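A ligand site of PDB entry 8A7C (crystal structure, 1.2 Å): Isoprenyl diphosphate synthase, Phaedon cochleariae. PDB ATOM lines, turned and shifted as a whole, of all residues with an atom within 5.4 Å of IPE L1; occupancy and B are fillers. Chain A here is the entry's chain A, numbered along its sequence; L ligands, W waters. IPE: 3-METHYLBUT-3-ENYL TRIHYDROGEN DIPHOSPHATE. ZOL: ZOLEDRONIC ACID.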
ATOM      1  N   GLY A  49     -33.912  19.076 -16.570  1.00  0.00           N
ATOM      2  CA  GLY A  49     -32.907  19.794 -15.782  1.00  0.00           C
ATOM      3  C   GLY A  49     -33.036  21.304 -15.951  1.00  0.00           C
ATOM      4  O   GLY A  49     -34.009  21.794 -16.529  1.00  0.00           O
ATOM      5  N   LYS A  50     -32.023  22.020 -15.487  1.00  0.00           N
ATOM      6  CA  LYS A  50     -32.050  23.506 -15.533  1.00  0.00           C
ATOM      7  C   LYS A  50     -31.764  24.030 -16.958  1.00  0.00           C
ATOM      8  O   LYS A  50     -32.098  25.178 -17.226  1.00  0.00           O
ATOM      9  CB  LYS A  50     -31.069  24.092 -14.529  1.00  0.00           C
ATOM     10  CG  LYS A  50     -31.368  23.727 -13.087  1.00  0.00           C
ATOM     11  CD  LYS A  50     -30.323  24.250 -12.128  1.00  0.00           C
ATOM     12  CE  LYS A  50     -28.946  23.726 -12.324  1.00  0.00           C
ATOM     13  NZ  LYS A  50     -28.943  22.383 -11.864  1.00  0.00           N
ATOM     14  N   LYS A  51     -31.131  23.233 -17.791  1.00  0.00           N
ATOM     15  CA  LYS A  51     -30.828  23.583 -19.201  1.00  0.00           C
ATOM     16  C   LYS A  51     -29.841  24.751 -19.284  1.00  0.00           C
ATOM     17  O   LYS A  51     -29.765  25.439 -20.331  1.00  0.00           O
ATOM     18  CB  LYS A  51     -32.133  23.793 -20.008  1.00  0.00           C
ATOM     19  CG  LYS A  51     -32.919  22.504 -20.149  1.00  0.00           C
ATOM     20  CD  LYS A  51     -34.326  22.640 -20.739  1.00  0.00           C
ATOM     21  CE  LYS A  51     -35.306  23.325 -19.847  1.00  0.00           C
ATOM     22  NZ  LYS A  51     -35.642  22.485 -18.701  1.00  0.00           N
ATOM     23  N   ARG A  53     -26.585  24.698 -19.759  1.00  0.00           N
ATOM     24  CA  ARG A  53     -25.636  24.481 -20.841  1.00  0.00           C
ATOM     25  C   ARG A  53     -26.273  24.817 -22.183  1.00  0.00           C
ATOM     26  O   ARG A  53     -25.647  25.561 -23.008  1.00  0.00           O
ATOM     27  CB  ARG A  53     -25.096  23.051 -20.851  1.00  0.00           C
ATOM     28  CG  ARG A  53     -24.317  22.650 -19.616  1.00  0.00           C
ATOM     29  CD  ARG A  53     -24.173  21.138 -19.520  1.00  0.00           C
ATOM     30  NE  ARG A  53     -23.558  20.701 -18.269  1.00  0.00           N
ATOM     31  CZ  ARG A  53     -24.151  20.723 -17.089  1.00  0.00           C
ATOM     32  NH1 ARG A  53     -25.395  21.126 -16.928  1.00  0.00           N
ATOM     33  NH2 ARG A  53     -23.444  20.342 -16.018  1.00  0.00           N
ATOM     34  N   GLU A  86     -27.225  19.309 -24.284  1.00  0.00           N
ATOM     35  CA  GLU A  86     -28.171  18.669 -23.349  1.00  0.00           C
ATOM     36  C   GLU A  86     -28.262  17.149 -23.574  1.00  0.00           C
ATOM     37  O   GLU A  86     -28.440  16.418 -22.569  1.00  0.00           O
ATOM     38  CB  GLU A  86     -29.526  19.346 -23.377  1.00  0.00           C
ATOM     39  CG  GLU A  86     -29.498  20.785 -22.880  1.00  0.00           C
ATOM     40  CD  GLU A  86     -29.127  20.982 -21.424  1.00  0.00           C
ATOM     41  OE1 GLU A  86     -29.369  20.021 -20.623  1.00  0.00           O
ATOM     42  OE2 GLU A  86     -28.640  22.067 -21.042  1.00  0.00           O
ATOM     43  N   GLN A  89     -25.139  15.851 -21.862  1.00  0.00           N
ATOM     44  CA  GLN A  89     -25.432  15.881 -20.427  1.00  0.00           C
ATOM     45  C   GLN A  89     -26.326  14.694 -20.034  1.00  0.00           C
ATOM     46  O   GLN A  89     -26.067  13.999 -19.013  1.00  0.00           O
ATOM     47  CB  GLN A  89     -26.078  17.220 -20.051  1.00  0.00           C
ATOM     48  CG  GLN A  89     -26.709  17.280 -18.658  1.00  0.00           C
ATOM     49  CD  GLN A  89     -25.720  17.372 -17.518  1.00  0.00           C
ATOM     50  OE1 GLN A  89     -24.607  16.840 -17.614  1.00  0.00           O
ATOM     51  NE2 GLN A  89     -26.112  18.016 -16.418  1.00  0.00           N
ATOM     52  N   LEU A  93     -25.323  11.731 -17.299  1.00  0.00           N
ATOM     53  CA  LEU A  93     -26.014  11.546 -16.001  1.00  0.00           C
ATOM     54  C   LEU A  93     -26.582  10.121 -15.864  1.00  0.00           C
ATOM     55  O   LEU A  93     -26.571   9.543 -14.751  1.00  0.00           O
ATOM     56  CB  LEU A  93     -27.082  12.587 -15.755  1.00  0.00           C
ATOM     57  CG  LEU A  93     -26.603  14.058 -15.784  1.00  0.00           C
ATOM     58  CD1 LEU A  93     -27.755  14.982 -15.377  1.00  0.00           C
ATOM     59  CD2 LEU A  93     -25.400  14.287 -14.885  1.00  0.00           C
ATOM     60  N   ARG A 105     -32.618  11.569  -9.457  1.00  0.00           N
ATOM     61  CA  ARG A 105     -32.052  12.525 -10.411  1.00  0.00           C
ATOM     62  C   ARG A 105     -33.188  13.422 -10.880  1.00  0.00           C
ATOM     63  O   ARG A 105     -34.208  12.898 -11.320  1.00  0.00           O
ATOM     64  CB  ARG A 105     -31.426  11.786 -11.586  1.00  0.00           C
ATOM     65  CG  ARG A 105     -30.991  12.690 -12.728  1.00  0.00           C
ATOM     66  CD  ARG A 105     -29.822  13.619 -12.413  1.00  0.00           C
ATOM     67  NE  ARG A 105     -28.600  12.877 -12.187  1.00  0.00           N
ATOM     68  CZ  ARG A 105     -27.450  13.440 -11.806  1.00  0.00           C
ATOM     69  NH1 ARG A 105     -27.359  14.757 -11.683  1.00  0.00           N
ATOM     70  NH2 ARG A 105     -26.371  12.689 -11.646  1.00  0.00           N
ATOM     71  N   ARG A 106     -33.007  14.728 -10.810  1.00  0.00           N
ATOM     72  CA  ARG A 106     -34.001  15.682 -11.314  1.00  0.00           C
ATOM     73  C   ARG A 106     -35.379  15.372 -10.730  1.00  0.00           C
ATOM     74  O   ARG A 106     -36.385  15.564 -11.373  1.00  0.00           O
ATOM     75  CB  ARG A 106     -33.975  15.732 -12.845  1.00  0.00           C
ATOM     76  CG  ARG A 106     -32.681  16.282 -13.414  1.00  0.00           C
ATOM     77  CD  ARG A 106     -32.626  16.046 -14.941  1.00  0.00           C
ATOM     78  NE  ARG A 106     -31.444  16.655 -15.521  1.00  0.00           N
ATOM     79  CZ  ARG A 106     -31.095  16.499 -16.809  1.00  0.00           C
ATOM     80  NH1 ARG A 106     -31.826  15.742 -17.608  1.00  0.00           N
ATOM     81  NH2 ARG A 106     -30.012  17.087 -17.250  1.00  0.00           N
ATOM     82  N   THR A 194     -15.961  17.789 -15.656  1.00  0.00           N
ATOM     83  CA  THR A 194     -17.030  18.816 -15.627  1.00  0.00           C
ATOM     84  C   THR A 194     -16.713  20.023 -16.543  1.00  0.00           C
ATOM     85  O   THR A 194     -17.591  20.434 -17.294  1.00  0.00           O
ATOM     86  CB  THR A 194     -17.317  19.280 -14.204  1.00  0.00           C
ATOM     87  OG1 THR A 194     -18.000  18.169 -13.593  1.00  0.00           O
ATOM     88  CG2 THR A 194     -18.143  20.546 -14.153  1.00  0.00           C
ATOM     89  N   TYR A 197     -17.104  20.000 -20.682  1.00  0.00           N
ATOM     90  CA  TYR A 197     -18.425  19.830 -21.314  1.00  0.00           C
ATOM     91  C   TYR A 197     -19.432  20.851 -20.817  1.00  0.00           C
ATOM     92  O   TYR A 197     -20.377  21.143 -21.558  1.00  0.00           O
ATOM     93  CB  TYR A 197     -18.940  18.407 -21.216  1.00  0.00           C
ATOM     94  CG  TYR A 197     -19.759  18.082 -19.987  1.00  0.00           C
ATOM     95  CD1 TYR A 197     -21.147  18.191 -20.025  1.00  0.00           C
ATOM     96  CD2 TYR A 197     -19.220  17.674 -18.765  1.00  0.00           C
ATOM     97  CE1 TYR A 197     -21.976  17.859 -18.963  1.00  0.00           C
ATOM     98  CE2 TYR A 197     -20.035  17.375 -17.676  1.00  0.00           C
ATOM     99  CZ  TYR A 197     -21.403  17.478 -17.775  1.00  0.00           C
ATOM    100  OH  TYR A 197     -22.158  17.137 -16.692  1.00  0.00           O
ATOM    101  N   THR A 198     -19.261  21.345 -19.593  1.00  0.00           N
ATOM    102  CA  THR A 198     -20.267  22.216 -19.016  1.00  0.00           C
ATOM    103  C   THR A 198     -20.058  23.683 -19.437  1.00  0.00           C
ATOM    104  O   THR A 198     -21.053  24.407 -19.607  1.00  0.00           O
ATOM    105  CB  THR A 198     -20.305  22.054 -17.490  1.00  0.00           C
ATOM    106  OG1 THR A 198     -20.645  20.692 -17.160  1.00  0.00           O
ATOM    107  CG2 THR A 198     -21.318  22.957 -16.817  1.00  0.00           C
ATOM    108  N   PHE A 232     -18.032  25.875 -10.095  1.00  0.00           N
ATOM    109  CA  PHE A 232     -19.338  25.208 -10.235  1.00  0.00           C
ATOM    110  C   PHE A 232     -19.320  23.813  -9.610  1.00  0.00           C
ATOM    111  O   PHE A 232     -20.319  23.373  -8.985  1.00  0.00           O
ATOM    112  CB  PHE A 232     -19.645  25.124 -11.725  1.00  0.00           C
ATOM    113  CG  PHE A 232     -20.967  24.475 -12.054  1.00  0.00           C
ATOM    114  CD1 PHE A 232     -22.166  25.154 -11.876  1.00  0.00           C
ATOM    115  CD2 PHE A 232     -21.009  23.178 -12.538  1.00  0.00           C
ATOM    116  CE1 PHE A 232     -23.360  24.563 -12.243  1.00  0.00           C
ATOM    117  CE2 PHE A 232     -22.208  22.610 -12.897  1.00  0.00           C
ATOM    118  CZ  PHE A 232     -23.381  23.286 -12.744  1.00  0.00           C
ATOM    119  N   GLN A 233     -18.252  23.042  -9.835  1.00  0.00           N
ATOM    120  CA  GLN A 233     -18.160  21.668  -9.265  1.00  0.00           C
ATOM    121  C   GLN A 233     -18.008  21.736  -7.748  1.00  0.00           C
ATOM    122  O   GLN A 233     -18.519  20.838  -7.046  1.00  0.00           O
ATOM    123  CB  GLN A 233     -17.041  20.870  -9.932  1.00  0.00           C
ATOM    124  CG  GLN A 233     -17.062  19.400  -9.500  1.00  0.00           C
ATOM    125  CD  GLN A 233     -18.321  18.679  -9.914  1.00  0.00           C
ATOM    126  OE1 GLN A 233     -18.768  18.756 -11.049  1.00  0.00           O
ATOM    127  NE2 GLN A 233     -18.874  17.935  -8.951  1.00  0.00           N
ATOM    128  N   ASP A 236     -21.376  21.993  -6.563  1.00  0.00           N
ATOM    129  CA  ASP A 236     -22.063  20.693  -6.661  1.00  0.00           C
ATOM    130  C   ASP A 236     -21.696  19.790  -5.455  1.00  0.00           C
ATOM    131  O   ASP A 236     -22.550  19.088  -4.909  1.00  0.00           O
ATOM    132  CB  ASP A 236     -21.709  19.974  -7.954  1.00  0.00           C
ATOM    133  CG  ASP A 236     -22.452  18.677  -8.133  1.00  0.00           C
ATOM    134  OD1 ASP A 236     -23.697  18.768  -8.273  1.00  0.00           O
ATOM    135  OD2 ASP A 236     -21.778  17.596  -8.102  1.00  0.00           O
ATOM    136  N   LYS A 250     -31.726  15.470  -6.177  1.00  0.00           N
ATOM    137  CA  LYS A 250     -30.834  14.313  -6.095  1.00  0.00           C
ATOM    138  C   LYS A 250     -30.367  14.131  -4.652  1.00  0.00           C
ATOM    139  O   LYS A 250     -30.094  15.067  -3.932  1.00  0.00           O
ATOM    140  CB  LYS A 250     -29.663  14.444  -7.072  1.00  0.00           C
ATOM    141  CG  LYS A 250     -28.732  15.618  -6.876  1.00  0.00           C
ATOM    142  CD  LYS A 250     -27.822  15.893  -8.093  1.00  0.00           C
ATOM    143  CE  LYS A 250     -26.714  16.846  -7.745  1.00  0.00           C
ATOM    144  NZ  LYS A 250     -25.878  17.192  -8.896  1.00  0.00           N
ATOM    145  N   ARG A 344     -26.271  29.510  -5.959  1.00  0.00           N
ATOM    146  CA  ARG A 344     -27.353  28.552  -6.302  1.00  0.00           C
ATOM    147  C   ARG A 344     -27.563  27.503  -5.199  1.00  0.00           C
ATOM    148  O   ARG A 344     -26.622  27.131  -4.471  1.00  0.00           O
ATOM    149  CB  ARG A 344     -27.005  27.858  -7.617  1.00  0.00           C
ATOM    150  CG  ARG A 344     -25.847  26.865  -7.586  1.00  0.00           C
ATOM    151  CD  ARG A 344     -25.458  26.472  -8.983  1.00  0.00           C
ATOM    152  NE  ARG A 344     -24.337  25.549  -9.028  1.00  0.00           N
ATOM    153  CZ  ARG A 344     -24.477  24.217  -9.034  1.00  0.00           C
ATOM    154  NH1 ARG A 344     -25.680  23.703  -9.117  1.00  0.00           N
ATOM    155  NH2 ARG A 344     -23.417  23.441  -9.081  1.00  0.00           N
ATOM    156  N   ALA A 346     -29.408  24.659  -6.230  1.00  0.00           N
ATOM    157  CA  ALA A 346     -29.783  23.524  -7.088  1.00  0.00           C
ATOM    158  C   ALA A 346     -28.937  23.565  -8.343  1.00  0.00           C
ATOM    159  O   ALA A 346     -28.804  22.541  -9.011  1.00  0.00           O
ATOM    160  CB  ALA A 346     -31.238  23.529  -7.455  1.00  0.00           C
ATOM    161  OXT ALA A 346     -28.375  24.663  -8.660  1.00  0.00           O
HETATM  162  C1  IPE L   1     -24.995  18.264 -12.866  1.00  0.00           C
HETATM  163  O1  IPE L   1     -25.258  19.425 -13.680  1.00  0.00           O
HETATM  164  C2  IPE L   1     -23.628  17.713 -13.143  1.00  0.00           C
HETATM  165  C3  IPE L   1     -22.494  18.683 -12.905  1.00  0.00           C
HETATM  166  C4  IPE L   1     -21.533  18.843 -13.794  1.00  0.00           C
HETATM  167  C5  IPE L   1     -22.467  19.344 -11.553  1.00  0.00           C
HETATM  168  PA  IPE L   1     -26.449  20.403 -13.353  1.00  0.00           P
HETATM  169  O1A IPE L   1     -26.485  20.697 -11.908  1.00  0.00           O
HETATM  170  O2A IPE L   1     -26.332  21.530 -14.330  1.00  0.00           O
HETATM  171  O3A IPE L   1     -27.715  19.500 -13.678  1.00  0.00           O
HETATM  172  PB  IPE L   1     -29.049  19.597 -14.622  1.00  0.00           P
HETATM  173  O1B IPE L   1     -30.026  18.580 -13.996  1.00  0.00           O
HETATM  174  O2B IPE L   1     -29.544  21.015 -14.484  1.00  0.00           O
HETATM  175  O3B IPE L   1     -28.631  19.226 -15.999  1.00  0.00           O
HETATM  176  O17 ZOL L   2     -19.482  14.227 -10.536  1.00  0.00           O
HETATM  177  P14 ZOL L   2     -20.772  13.952  -9.815  1.00  0.00           P
HETATM  178  O16 ZOL L   2     -21.153  12.435  -9.845  1.00  0.00           O
HETATM  179  O15 ZOL L   2     -20.785  14.544  -8.401  1.00  0.00           O
HETATM  180  C8  ZOL L   2     -22.148  14.829 -10.699  1.00  0.00           C
HETATM  181  P9  ZOL L   2     -23.764  14.605  -9.819  1.00  0.00           P
HETATM  182  O10 ZOL L   2     -23.600  15.271  -8.484  1.00  0.00           O
HETATM  183  O11 ZOL L   2     -24.028  13.116  -9.678  1.00  0.00           O
HETATM  184  O12 ZOL L   2     -24.820  15.292 -10.677  1.00  0.00           O
HETATM  185  O13 ZOL L   2     -21.847  16.238 -10.698  1.00  0.00           O
HETATM  186  C7  ZOL L   2     -22.274  14.366 -12.150  1.00  0.00           C
HETATM  187  N15 ZOL L   2     -21.075  14.628 -12.969  1.00  0.00           N
HETATM  188  C16 ZOL L   2     -20.401  15.795 -13.133  1.00  0.00           C
HETATM  189  N17 ZOL L   2     -19.407  15.637 -13.960  1.00  0.00           N
HETATM  190  C18 ZOL L   2     -19.400  14.344 -14.358  1.00  0.00           C
HETATM  191  C19 ZOL L   2     -20.451  13.698 -13.767  1.00  0.00           C
HETATM  192  O   HOH W   1     -28.343  22.837 -16.201  1.00  0.00           O
HETATM  193  O   HOH W   2     -30.120  20.489 -18.017  1.00  0.00           O
HETATM  194  O   HOH W   3     -29.173  17.067 -11.845  1.00  0.00           O
HETATM  195  O   HOH W   4     -24.895  20.924  -9.522  1.00  0.00           O
HETATM  196  O   HOH W   5     -26.218  24.239 -14.539  1.00  0.00           O
HETATM  197  O   HOH W   6     -31.695  19.839 -12.154  1.00  0.00           O
HETATM  198  O   HOH W   7     -27.695  18.820 -10.333  1.00  0.00           O
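The side-chain amino group of Lys 50 lies within salt-bridge range of an oxygen (O1A) of IPE L1 (3.0 Å).
The guanidinium group (NE) of Arg 106 lies within salt-bridge range of an oxygen (O1B) of IPE L1 (2.8 Å).
The side-chain hydroxyl of Thr 194 sits at hydrogen-bond distance from a nitrogen (N17) of ZOL L2 (2.9 Å).
An oxygen (O12) of ZOL L2 is in salt-bridge range of the side-chain amino group (NZ) of Lys 250, at 2.8 Å.
An oxygen (O2B) of IPE L1 lies within hydrogen-bond range of the backbone NH of Lys 50 (2.9 Å).
The guanidinium group (NH1) of Arg 105 is in salt-bridge range of an oxygen (O12) of ZOL L2 (2.8 Å).
O2A of IPE L1 is in salt-bridge range of NH1 of Arg 53 (2.8 Å).
The side-chain amide nitrogen (NE2) of Gln 89 sits at hydrogen-bond distance from an oxygen (O3B) of IPE L1 (2.8 Å).
The side-chain carboxylate (OD1) of Asp 236 is in salt-bridge range of the side-chain amino group (NZ) of Lys 250.
The side-chain hydroxyl of Tyr 197 sits at hydrogen-bond distance from the side-chain amide oxygen of Gln 89, 2.6 Å away.
NE2 of Gln 89 lies close to NH1 of Arg 53 (3.2 Å).
The side-chain amide nitrogen of Gln 233 sits close to the side-chain carboxylate of Asp 236 (3.0 Å).
The side-chain hydroxyl (OG1) of Thr 198 sits at hydrogen-bond distance from the guanidinium group (NH2) of Arg 53.
The backbone carbonyl oxygen (O) of Phe 232 lies within hydrogen-bond range of the guanidinium group (NH2) of Arg 344 (3.1 Å).
The backbone carbonyl oxygen (O) of Gly 49 lies within hydrogen-bond range of the side-chain amino group (NZ) of Lys 51, 2.8 Å away.
The side-chain amide oxygen (OE1) of Gln 233 is in hydrogen-bond range of the side-chain hydroxyl (OG1) of Thr 194 (2.7 Å).
Residues that only touch IPE L1: Tyr 197 (3.4 Å), Asp 236 (3.5 Å), Phe 232 (3.5 Å), Gly 49 (3.6 Å), Thr 194 (3.6 Å), Gln 233 (3.8 Å) and Thr 198 (3.9 Å).
Of the 18 residues printed, 11 come within 4 Å of IPE L1.
The nearest printed residue that does not touch IPE L1 is Ala 346 (4.1 Å).
Water W7 lies within hydrogen-bond range of O1A of IPE L1 (2.7 Å) and NZ of Lys 250 (2.8 Å).
Water W3 lies within hydrogen-bond range of an oxygen (O1B) of IPE L1 (2.8 Å) and the guanidinium group of Arg 105 (2.9 Å).
Water W1 lies within hydrogen-bond range of an oxygen (O2B) of IPE L1, the backbone NH of Lys 51 and the guanidinium group of Arg 53.
Water W2 lies within hydrogen-bond range of the side-chain carboxylate of Glu 86 (2.8 Å), an oxygen (O3B) of IPE L1 (2.8 Å), the backbone NH of Lys 51 (2.9 Å) and the guanidinium group of Arg 106 (3.5 Å).
Water W4 lies within hydrogen-bond range of the side-chain carboxylate of Asp 236 (2.8 Å), an oxygen (O1A) of IPE L1 (2.9 Å) and the guanidinium group of Arg 344 (2.9 Å).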
